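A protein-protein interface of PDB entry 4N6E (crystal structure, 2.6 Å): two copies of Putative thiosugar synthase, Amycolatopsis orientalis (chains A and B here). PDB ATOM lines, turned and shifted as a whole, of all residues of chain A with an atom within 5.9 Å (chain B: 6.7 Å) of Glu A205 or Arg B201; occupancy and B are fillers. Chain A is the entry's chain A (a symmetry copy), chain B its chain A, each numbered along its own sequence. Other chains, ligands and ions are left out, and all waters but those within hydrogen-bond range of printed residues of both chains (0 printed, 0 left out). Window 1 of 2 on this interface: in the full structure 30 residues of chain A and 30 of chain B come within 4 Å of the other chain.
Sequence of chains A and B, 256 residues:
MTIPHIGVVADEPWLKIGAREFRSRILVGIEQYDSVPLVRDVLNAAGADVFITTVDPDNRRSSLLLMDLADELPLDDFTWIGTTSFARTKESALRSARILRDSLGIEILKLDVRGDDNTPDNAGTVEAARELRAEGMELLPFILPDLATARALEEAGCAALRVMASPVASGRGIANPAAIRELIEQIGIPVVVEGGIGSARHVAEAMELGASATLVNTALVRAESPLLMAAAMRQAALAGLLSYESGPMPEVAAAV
The side-chain hydroxyl (OG) of Ser B199 is in hydrogen-bond range of the side-chain carboxylate (OE2) of Glu A208 (2.7 Å).
OE1 of Glu A208 sits at hydrogen-bond distance from N of Ala B200.
OG of Ser A243 sits at hydrogen-bond distance from N of Ala B200 (3.5 Å).
The guanidinium group (NH1) of Arg B201 is in salt-bridge range of the side-chain carboxylate (OE2) of Glu A208 (2.6 Å).
The side-chain hydroxyl of Ser A243 lies close to the side-chain sulfur of Met B229, 3.6 Å away.
The side-chain hydroxyl (OG) of Ser B199 lies within hydrogen-bond range of the guanidinium group (NH1) of Arg B201 (3.3 Å).
N of Ser B199 sits at hydrogen-bond distance from ND1 of His B202, at 3.4 Å.
The side-chain hydroxyl of Ser A243 is in hydrogen-bond range of the side-chain carboxylate of Glu A208, at 2.8 Å.
Among the printed residues, merely in contact across the chains: Arg A201 with Glu B205 (3.6 Å), Glu A205 with Arg B201 (3.6 Å) and Ser A243 with Ser B199 (3.7 Å).
Of chain B, only Arg B201 comes within 4 Å of Glu A205.
Ala A206 touches none of the printed residues of chain B.
Of the printed residues of chain A, Ser B199 touches Glu A208 and Ser A243.
Arg B201 touches just these residues of chain A: Glu A205 and Glu A208.
Val B203 touches none of the printed residues of chain A.
Of the printed residues of chain A, Glu B205 touches Arg A201.
The nearest residue of chain A that does not touch Arg B201 is Ala A204 (4.04 Å).
Printed residues of chain B that touch a printed residue of chain A: Ser B199, Ala B200, Arg B201, Glu B205 and Met B229.
Among the printed residues, Asp or Glu carboxylates within 4 Å of a Lys or Arg side-chain nitrogen of the other chain: Glu A208 with Arg B201 (2.6 Å).
Arg A201 touches Glu B205, and with the chains exchanged Glu A205 touches Arg B201.
Positions printed for both chains: 174, 200, 201, 202, 203, 204, 205 and 206.
Of the 8 pairs that touch across the chains among the printed residues, 2 have their exchanged pair printed and touching as well.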
ATOM      1  N   GLY A 173       3.733  -1.567  18.923  1.00  0.00           N
ATOM      2  CA  GLY A 173       4.321  -2.840  19.304  1.00  0.00           C
ATOM      3  C   GLY A 173       3.305  -3.836  19.872  1.00  0.00           C
ATOM      4  O   GLY A 173       2.219  -4.019  19.316  1.00  0.00           O
ATOM      5  N   ILE A 174       3.667  -4.463  20.992  1.00  0.00           N
ATOM      6  CA  ILE A 174       2.895  -5.543  21.597  1.00  0.00           C
ATOM      7  C   ILE A 174       2.124  -5.067  22.843  1.00  0.00           C
ATOM      8  O   ILE A 174       2.702  -4.827  23.900  1.00  0.00           O
ATOM      9  CB  ILE A 174       3.837  -6.707  21.950  1.00  0.00           C
ATOM     10  CG1 ILE A 174       4.767  -6.980  20.764  1.00  0.00           C
ATOM     11  CG2 ILE A 174       3.030  -7.925  22.328  1.00  0.00           C
ATOM     12  CD1 ILE A 174       5.588  -8.243  20.839  1.00  0.00           C
ATOM     13  N   PRO A 177       1.612  -8.537  26.063  1.00  0.00           N
ATOM     14  CA  PRO A 177       2.581  -9.603  25.829  1.00  0.00           C
ATOM     15  C   PRO A 177       2.310 -10.897  26.597  1.00  0.00           C
ATOM     16  O   PRO A 177       2.616 -11.970  26.097  1.00  0.00           O
ATOM     17  CB  PRO A 177       3.921  -8.976  26.267  1.00  0.00           C
ATOM     18  CG  PRO A 177       3.562  -7.797  27.093  1.00  0.00           C
ATOM     19  CD  PRO A 177       2.270  -7.301  26.526  1.00  0.00           C
ATOM     20  N   ALA A 200      12.263  -2.703  14.795  1.00  0.00           N
ATOM     21  CA  ALA A 200      13.021  -3.932  15.016  1.00  0.00           C
ATOM     22  C   ALA A 200      12.967  -4.431  16.453  1.00  0.00           C
ATOM     23  O   ALA A 200      13.002  -5.638  16.706  1.00  0.00           O
ATOM     24  CB  ALA A 200      14.479  -3.736  14.587  1.00  0.00           C
ATOM     25  N   ARG A 201      12.873  -3.520  17.410  1.00  0.00           N
ATOM     26  CA  ARG A 201      12.836  -3.954  18.805  1.00  0.00           C
ATOM     27  C   ARG A 201      11.539  -4.702  19.060  1.00  0.00           C
ATOM     28  O   ARG A 201      11.496  -5.609  19.905  1.00  0.00           O
ATOM     29  CB  ARG A 201      13.033  -2.792  19.785  1.00  0.00           C
ATOM     30  CG  ARG A 201      11.755  -2.140  20.284  1.00  0.00           C
ATOM     31  CD  ARG A 201      12.071  -1.149  21.392  1.00  0.00           C
ATOM     32  NE  ARG A 201      10.948  -0.289  21.774  1.00  0.00           N
ATOM     33  CZ  ARG A 201      10.484   0.719  21.043  1.00  0.00           C
ATOM     34  NH1 ARG A 201      11.024   0.994  19.870  1.00  0.00           N
ATOM     35  NH2 ARG A 201       9.458   1.445  21.480  1.00  0.00           N
ATOM     36  N   HIS A 202      10.490  -4.342  18.324  1.00  0.00           N
ATOM     37  CA  HIS A 202       9.201  -5.062  18.454  1.00  0.00           C
ATOM     38  C   HIS A 202       9.251  -6.486  17.924  1.00  0.00           C
ATOM     39  O   HIS A 202       8.538  -7.347  18.410  1.00  0.00           O
ATOM     40  CB  HIS A 202       8.071  -4.298  17.773  1.00  0.00           C
ATOM     41  CG  HIS A 202       7.756  -2.994  18.434  1.00  0.00           C
ATOM     42  ND1 HIS A 202       7.188  -1.938  17.761  1.00  0.00           N
ATOM     43  CD2 HIS A 202       7.961  -2.568  19.704  1.00  0.00           C
ATOM     44  CE1 HIS A 202       7.021  -0.925  18.590  1.00  0.00           C
ATOM     45  NE2 HIS A 202       7.495  -1.277  19.773  1.00  0.00           N
ATOM     46  N   VAL A 203      10.096  -6.719  16.921  1.00  0.00           N
ATOM     47  CA  VAL A 203      10.278  -8.055  16.354  1.00  0.00           C
ATOM     48  C   VAL A 203      10.955  -8.963  17.391  1.00  0.00           C
ATOM     49  O   VAL A 203      10.482 -10.079  17.697  1.00  0.00           O
ATOM     50  CB  VAL A 203      11.160  -8.002  15.106  1.00  0.00           C
ATOM     51  CG1 VAL A 203      11.520  -9.420  14.655  1.00  0.00           C
ATOM     52  CG2 VAL A 203      10.476  -7.209  13.996  1.00  0.00           C
ATOM     53  N   ALA A 204      12.068  -8.473  17.914  1.00  0.00           N
ATOM     54  CA  ALA A 204      12.817  -9.201  18.892  1.00  0.00           C
ATOM     55  C   ALA A 204      11.931  -9.497  20.105  1.00  0.00           C
ATOM     56  O   ALA A 204      11.936 -10.625  20.618  1.00  0.00           O
ATOM     57  CB  ALA A 204      14.067  -8.415  19.283  1.00  0.00           C
ATOM     58  N   GLU A 205      11.152  -8.506  20.544  1.00  0.00           N
ATOM     59  CA  GLU A 205      10.152  -8.741  21.617  1.00  0.00           C
ATOM     60  C   GLU A 205       9.190  -9.877  21.205  1.00  0.00           C
ATOM     61  O   GLU A 205       9.002 -10.827  21.944  1.00  0.00           O
ATOM     62  CB  GLU A 205       9.381  -7.450  21.965  1.00  0.00           C
ATOM     63  CG  GLU A 205       8.489  -7.546  23.198  1.00  0.00           C
ATOM     64  CD  GLU A 205       7.670  -6.281  23.480  1.00  0.00           C
ATOM     65  OE1 GLU A 205       6.938  -6.245  24.495  1.00  0.00           O
ATOM     66  OE2 GLU A 205       7.745  -5.312  22.700  1.00  0.00           O
ATOM     67  N   ALA A 206       8.633  -9.809  20.003  1.00  0.00           N
ATOM     68  CA  ALA A 206       7.731 -10.878  19.538  1.00  0.00           C
ATOM     69  C   ALA A 206       8.358 -12.276  19.639  1.00  0.00           C
ATOM     70  O   ALA A 206       7.693 -13.209  20.081  1.00  0.00           O
ATOM     71  CB  ALA A 206       7.237 -10.610  18.131  1.00  0.00           C
ATOM     72  N   MET A 207       9.641 -12.390  19.277  1.00  0.00           N
ATOM     73  CA  MET A 207      10.344 -13.683  19.232  1.00  0.00           C
ATOM     74  C   MET A 207      10.682 -14.188  20.629  1.00  0.00           C
ATOM     75  O   MET A 207      10.679 -15.387  20.905  1.00  0.00           O
ATOM     76  CB  MET A 207      11.643 -13.565  18.422  1.00  0.00           C
ATOM     77  CG  MET A 207      11.484 -13.162  16.956  1.00  0.00           C
ATOM     78  SD  MET A 207      10.339 -14.185  15.997  1.00  0.00           S
ATOM     79  CE  MET A 207      11.447 -15.457  15.410  1.00  0.00           C
ATOM     80  N   GLU A 208      10.977 -13.261  21.527  1.00  0.00           N
ATOM     81  CA  GLU A 208      11.213 -13.635  22.913  1.00  0.00           C
ATOM     82  C   GLU A 208       9.955 -14.077  23.653  1.00  0.00           C
ATOM     83  O   GLU A 208      10.067 -14.673  24.728  1.00  0.00           O
ATOM     84  CB  GLU A 208      11.900 -12.505  23.648  1.00  0.00           C
ATOM     85  CG  GLU A 208      13.336 -12.305  23.207  1.00  0.00           C
ATOM     86  CD  GLU A 208      14.033 -11.283  24.075  1.00  0.00           C
ATOM     87  OE1 GLU A 208      15.156 -10.851  23.717  1.00  0.00           O
ATOM     88  OE2 GLU A 208      13.443 -10.919  25.120  1.00  0.00           O
ATOM     89  N   LEU A 209       8.774 -13.796  23.097  1.00  0.00           N
ATOM     90  CA  LEU A 209       7.521 -14.411  23.599  1.00  0.00           C
ATOM     91  C   LEU A 209       7.268 -15.827  23.043  1.00  0.00           C
ATOM     92  O   LEU A 209       6.350 -16.514  23.492  1.00  0.00           O
ATOM     93  CB  LEU A 209       6.310 -13.534  23.278  1.00  0.00           C
ATOM     94  CG  LEU A 209       6.373 -12.096  23.785  1.00  0.00           C
ATOM     95  CD1 LEU A 209       5.248 -11.270  23.180  1.00  0.00           C
ATOM     96  CD2 LEU A 209       6.342 -12.062  25.297  1.00  0.00           C
ATOM     97  N   GLY A 210       8.068 -16.243  22.062  1.00  0.00           N
ATOM     98  CA  GLY A 210       7.976 -17.574  21.465  1.00  0.00           C
ATOM     99  C   GLY A 210       7.424 -17.589  20.048  1.00  0.00           C
ATOM    100  O   GLY A 210       7.101 -18.661  19.528  1.00  0.00           O
ATOM    101  N   GLY A 240      16.212 -12.156  17.851  1.00  0.00           N
ATOM    102  CA  GLY A 240      15.074 -12.481  18.707  1.00  0.00           C
ATOM    103  C   GLY A 240      14.960 -13.962  18.978  1.00  0.00           C
ATOM    104  O   GLY A 240      14.699 -14.379  20.109  1.00  0.00           O
ATOM    105  N   SER A 243      17.848 -15.305  21.189  1.00  0.00           N
ATOM    106  CA  SER A 243      17.632 -14.838  22.551  1.00  0.00           C
ATOM    107  C   SER A 243      16.665 -15.778  23.238  1.00  0.00           C
ATOM    108  O   SER A 243      16.948 -16.308  24.318  1.00  0.00           O
ATOM    109  CB  SER A 243      17.081 -13.424  22.535  1.00  0.00           C
ATOM    110  OG  SER A 243      16.997 -12.896  23.845  1.00  0.00           O
ATOM    111  N   GLY B 171      17.538  -7.401  35.377  1.00  0.00           N
ATOM    112  CA  GLY B 171      16.925  -7.884  34.147  1.00  0.00           C
ATOM    113  C   GLY B 171      15.691  -7.120  33.694  1.00  0.00           C
ATOM    114  O   GLY B 171      14.919  -7.634  32.877  1.00  0.00           O
ATOM    115  N   ARG B 172      15.503  -5.901  34.198  1.00  0.00           N
ATOM    116  CA  ARG B 172      14.264  -5.149  33.950  1.00  0.00           C
ATOM    117  C   ARG B 172      14.334  -4.325  32.664  1.00  0.00           C
ATOM    118  O   ARG B 172      13.383  -3.621  32.345  1.00  0.00           O
ATOM    119  CB  ARG B 172      13.917  -4.189  35.122  1.00  0.00           C
ATOM    120  CG  ARG B 172      13.855  -4.815  36.520  1.00  0.00           C
ATOM    121  CD  ARG B 172      12.872  -4.149  37.497  1.00  0.00           C
ATOM    122  NE  ARG B 172      13.378  -2.953  38.190  1.00  0.00           N
ATOM    123  CZ  ARG B 172      13.132  -1.674  37.843  1.00  0.00           C
ATOM    124  NH1 ARG B 172      13.650  -0.686  38.576  1.00  0.00           N
ATOM    125  NH2 ARG B 172      12.386  -1.353  36.774  1.00  0.00           N
ATOM    126  N   ILE B 174      15.076  -1.240  30.330  1.00  0.00           N
ATOM    127  CA  ILE B 174      15.198   0.212  30.390  1.00  0.00           C
ATOM    128  C   ILE B 174      14.018   0.856  31.141  1.00  0.00           C
ATOM    129  O   ILE B 174      12.900   0.926  30.637  1.00  0.00           O
ATOM    130  CB  ILE B 174      15.306   0.774  28.961  1.00  0.00           C
ATOM    131  CG1 ILE B 174      16.312  -0.063  28.165  1.00  0.00           C
ATOM    132  CG2 ILE B 174      15.697   2.231  29.010  1.00  0.00           C
ATOM    133  CD1 ILE B 174      16.727   0.491  26.825  1.00  0.00           C
ATOM    134  N   GLY B 198      18.558  -7.430  30.373  1.00  0.00           N
ATOM    135  CA  GLY B 198      18.141  -8.816  30.564  1.00  0.00           C
ATOM    136  C   GLY B 198      18.158  -9.688  29.321  1.00  0.00           C
ATOM    137  O   GLY B 198      18.387 -10.889  29.427  1.00  0.00           O
ATOM    138  N   SER B 199      17.923  -9.107  28.142  1.00  0.00           N
ATOM    139  CA  SER B 199      17.876  -9.887  26.908  1.00  0.00           C
ATOM    140  C   SER B 199      18.119  -9.049  25.675  1.00  0.00           C
ATOM    141  O   SER B 199      18.232  -7.832  25.766  1.00  0.00           O
ATOM    142  CB  SER B 199      16.526 -10.588  26.757  1.00  0.00           C
ATOM    143  OG  SER B 199      15.510  -9.683  26.403  1.00  0.00           O
ATOM    144  N   ALA B 200      18.200  -9.724  24.526  1.00  0.00           N
ATOM    145  CA  ALA B 200      18.482  -9.091  23.241  1.00  0.00           C
ATOM    146  C   ALA B 200      17.494  -7.994  22.870  1.00  0.00           C
ATOM    147  O   ALA B 200      17.853  -7.013  22.215  1.00  0.00           O
ATOM    148  CB  ALA B 200      18.526 -10.148  22.132  1.00  0.00           C
ATOM    149  N   ARG B 201      16.245  -8.134  23.289  1.00  0.00           N
ATOM    150  CA  ARG B 201      15.258  -7.113  22.941  1.00  0.00           C
ATOM    151  C   ARG B 201      15.606  -5.821  23.658  1.00  0.00           C
ATOM    152  O   ARG B 201      15.323  -4.726  23.148  1.00  0.00           O
ATOM    153  CB  ARG B 201      13.823  -7.565  23.230  1.00  0.00           C
ATOM    154  CG  ARG B 201      13.281  -7.173  24.594  1.00  0.00           C
ATOM    155  CD  ARG B 201      11.798  -7.495  24.681  1.00  0.00           C
ATOM    156  NE  ARG B 201      11.232  -7.385  26.028  1.00  0.00           N
ATOM    157  CZ  ARG B 201      11.449  -8.252  27.012  1.00  0.00           C
ATOM    158  NH1 ARG B 201      12.242  -9.291  26.821  1.00  0.00           N
ATOM    159  NH2 ARG B 201      10.885  -8.067  28.202  1.00  0.00           N
ATOM    160  N   HIS B 202      16.233  -5.938  24.827  1.00  0.00           N
ATOM    161  CA  HIS B 202      16.673  -4.731  25.566  1.00  0.00           C
ATOM    162  C   HIS B 202      17.808  -3.988  24.882  1.00  0.00           C
ATOM    163  O   HIS B 202      17.918  -2.781  25.014  1.00  0.00           O
ATOM    164  CB  HIS B 202      17.070  -5.075  26.998  1.00  0.00           C
ATOM    165  CG  HIS B 202      15.921  -5.539  27.835  1.00  0.00           C
ATOM    166  ND1 HIS B 202      16.081  -6.362  28.926  1.00  0.00           N
ATOM    167  CD2 HIS B 202      14.590  -5.319  27.719  1.00  0.00           C
ATOM    168  CE1 HIS B 202      14.905  -6.604  29.472  1.00  0.00           C
ATOM    169  NE2 HIS B 202      13.981  -5.994  28.750  1.00  0.00           N
ATOM    170  N   VAL B 203      18.650  -4.723  24.158  1.00  0.00           N
ATOM    171  CA  VAL B 203      19.755  -4.124  23.408  1.00  0.00           C
ATOM    172  C   VAL B 203      19.193  -3.283  22.254  1.00  0.00           C
ATOM    173  O   VAL B 203      19.542  -2.095  22.074  1.00  0.00           O
ATOM    174  CB  VAL B 203      20.664  -5.205  22.821  1.00  0.00           C
ATOM    175  CG1 VAL B 203      21.680  -4.576  21.865  1.00  0.00           C
ATOM    176  CG2 VAL B 203      21.346  -5.996  23.934  1.00  0.00           C
ATOM    177  N   ALA B 204      18.329  -3.915  21.476  1.00  0.00           N
ATOM    178  CA  ALA B 204      17.718  -3.267  20.355  1.00  0.00           C
ATOM    179  C   ALA B 204      16.958  -2.026  20.829  1.00  0.00           C
ATOM    180  O   ALA B 204      17.059  -0.959  20.207  1.00  0.00           O
ATOM    181  CB  ALA B 204      16.805  -4.245  19.620  1.00  0.00           C
ATOM    182  N   GLU B 205      16.225  -2.150  21.937  1.00  0.00           N
ATOM    183  CA  GLU B 205      15.573  -0.967  22.556  1.00  0.00           C
ATOM    184  C   GLU B 205      16.629   0.115  22.872  1.00  0.00           C
ATOM    185  O   GLU B 205      16.480   1.258  22.477  1.00  0.00           O
ATOM    186  CB  GLU B 205      14.772  -1.357  23.817  1.00  0.00           C
ATOM    187  CG  GLU B 205      13.898  -0.248  24.392  1.00  0.00           C
ATOM    188  CD  GLU B 205      13.175  -0.628  25.690  1.00  0.00           C
ATOM    189  OE1 GLU B 205      12.399   0.201  26.218  1.00  0.00           O
ATOM    190  OE2 GLU B 205      13.367  -1.750  26.196  1.00  0.00           O
ATOM    191  N   ALA B 206      17.720  -0.259  23.528  1.00  0.00           N
ATOM    192  CA  ALA B 206      18.779   0.720  23.832  1.00  0.00           C
ATOM    193  C   ALA B 206      19.267   1.478  22.588  1.00  0.00           C
ATOM    194  O   ALA B 206      19.442   2.692  22.648  1.00  0.00           O
ATOM    195  CB  ALA B 206      19.940   0.069  24.555  1.00  0.00           C
ATOM    196  N   MET B 229      22.996 -16.431  24.103  1.00  0.00           N
ATOM    197  CA  MET B 229      22.587 -15.069  24.419  1.00  0.00           C
ATOM    198  C   MET B 229      23.651 -14.070  23.970  1.00  0.00           C
ATOM    199  O   MET B 229      23.317 -13.005  23.465  1.00  0.00           O
ATOM    200  CB  MET B 229      22.246 -14.885  25.896  1.00  0.00           C
ATOM    201  CG  MET B 229      21.781 -13.468  26.251  1.00  0.00           C
ATOM    202  SD  MET B 229      20.276 -12.893  25.432  1.00  0.00           S
ATOM    203  CE  MET B 229      19.062 -13.720  26.453  1.00  0.00           C
ATOM    204  N   MET B 233      22.746 -11.008  21.364  1.00  0.00           N
ATOM    205  CA  MET B 233      22.977  -9.574  21.668  1.00  0.00           C
ATOM    206  C   MET B 233      23.890  -8.889  20.668  1.00  0.00           C
ATOM    207  O   MET B 233      23.708  -7.710  20.343  1.00  0.00           O
ATOM    208  CB  MET B 233      23.552  -9.396  23.066  1.00  0.00           C
ATOM    209  CG  MET B 233      22.724 -10.089  24.118  1.00  0.00           C
ATOM    210  SD  MET B 233      22.890  -9.471  25.780  1.00  0.00           S
ATOM    211  CE  MET B 233      21.272  -8.778  25.998  1.00  0.00           C
ATOM    212  N   ALA B 236      21.424  -8.368  17.996  1.00  0.00           N
ATOM    213  CA  ALA B 236      20.482  -7.307  18.424  1.00  0.00           C
ATOM    214  C   ALA B 236      21.077  -5.918  18.324  1.00  0.00           C
ATOM    215  O   ALA B 236      20.340  -4.972  18.004  1.00  0.00           O
ATOM    216  CB  ALA B 236      20.004  -7.531  19.847  1.00  0.00           C
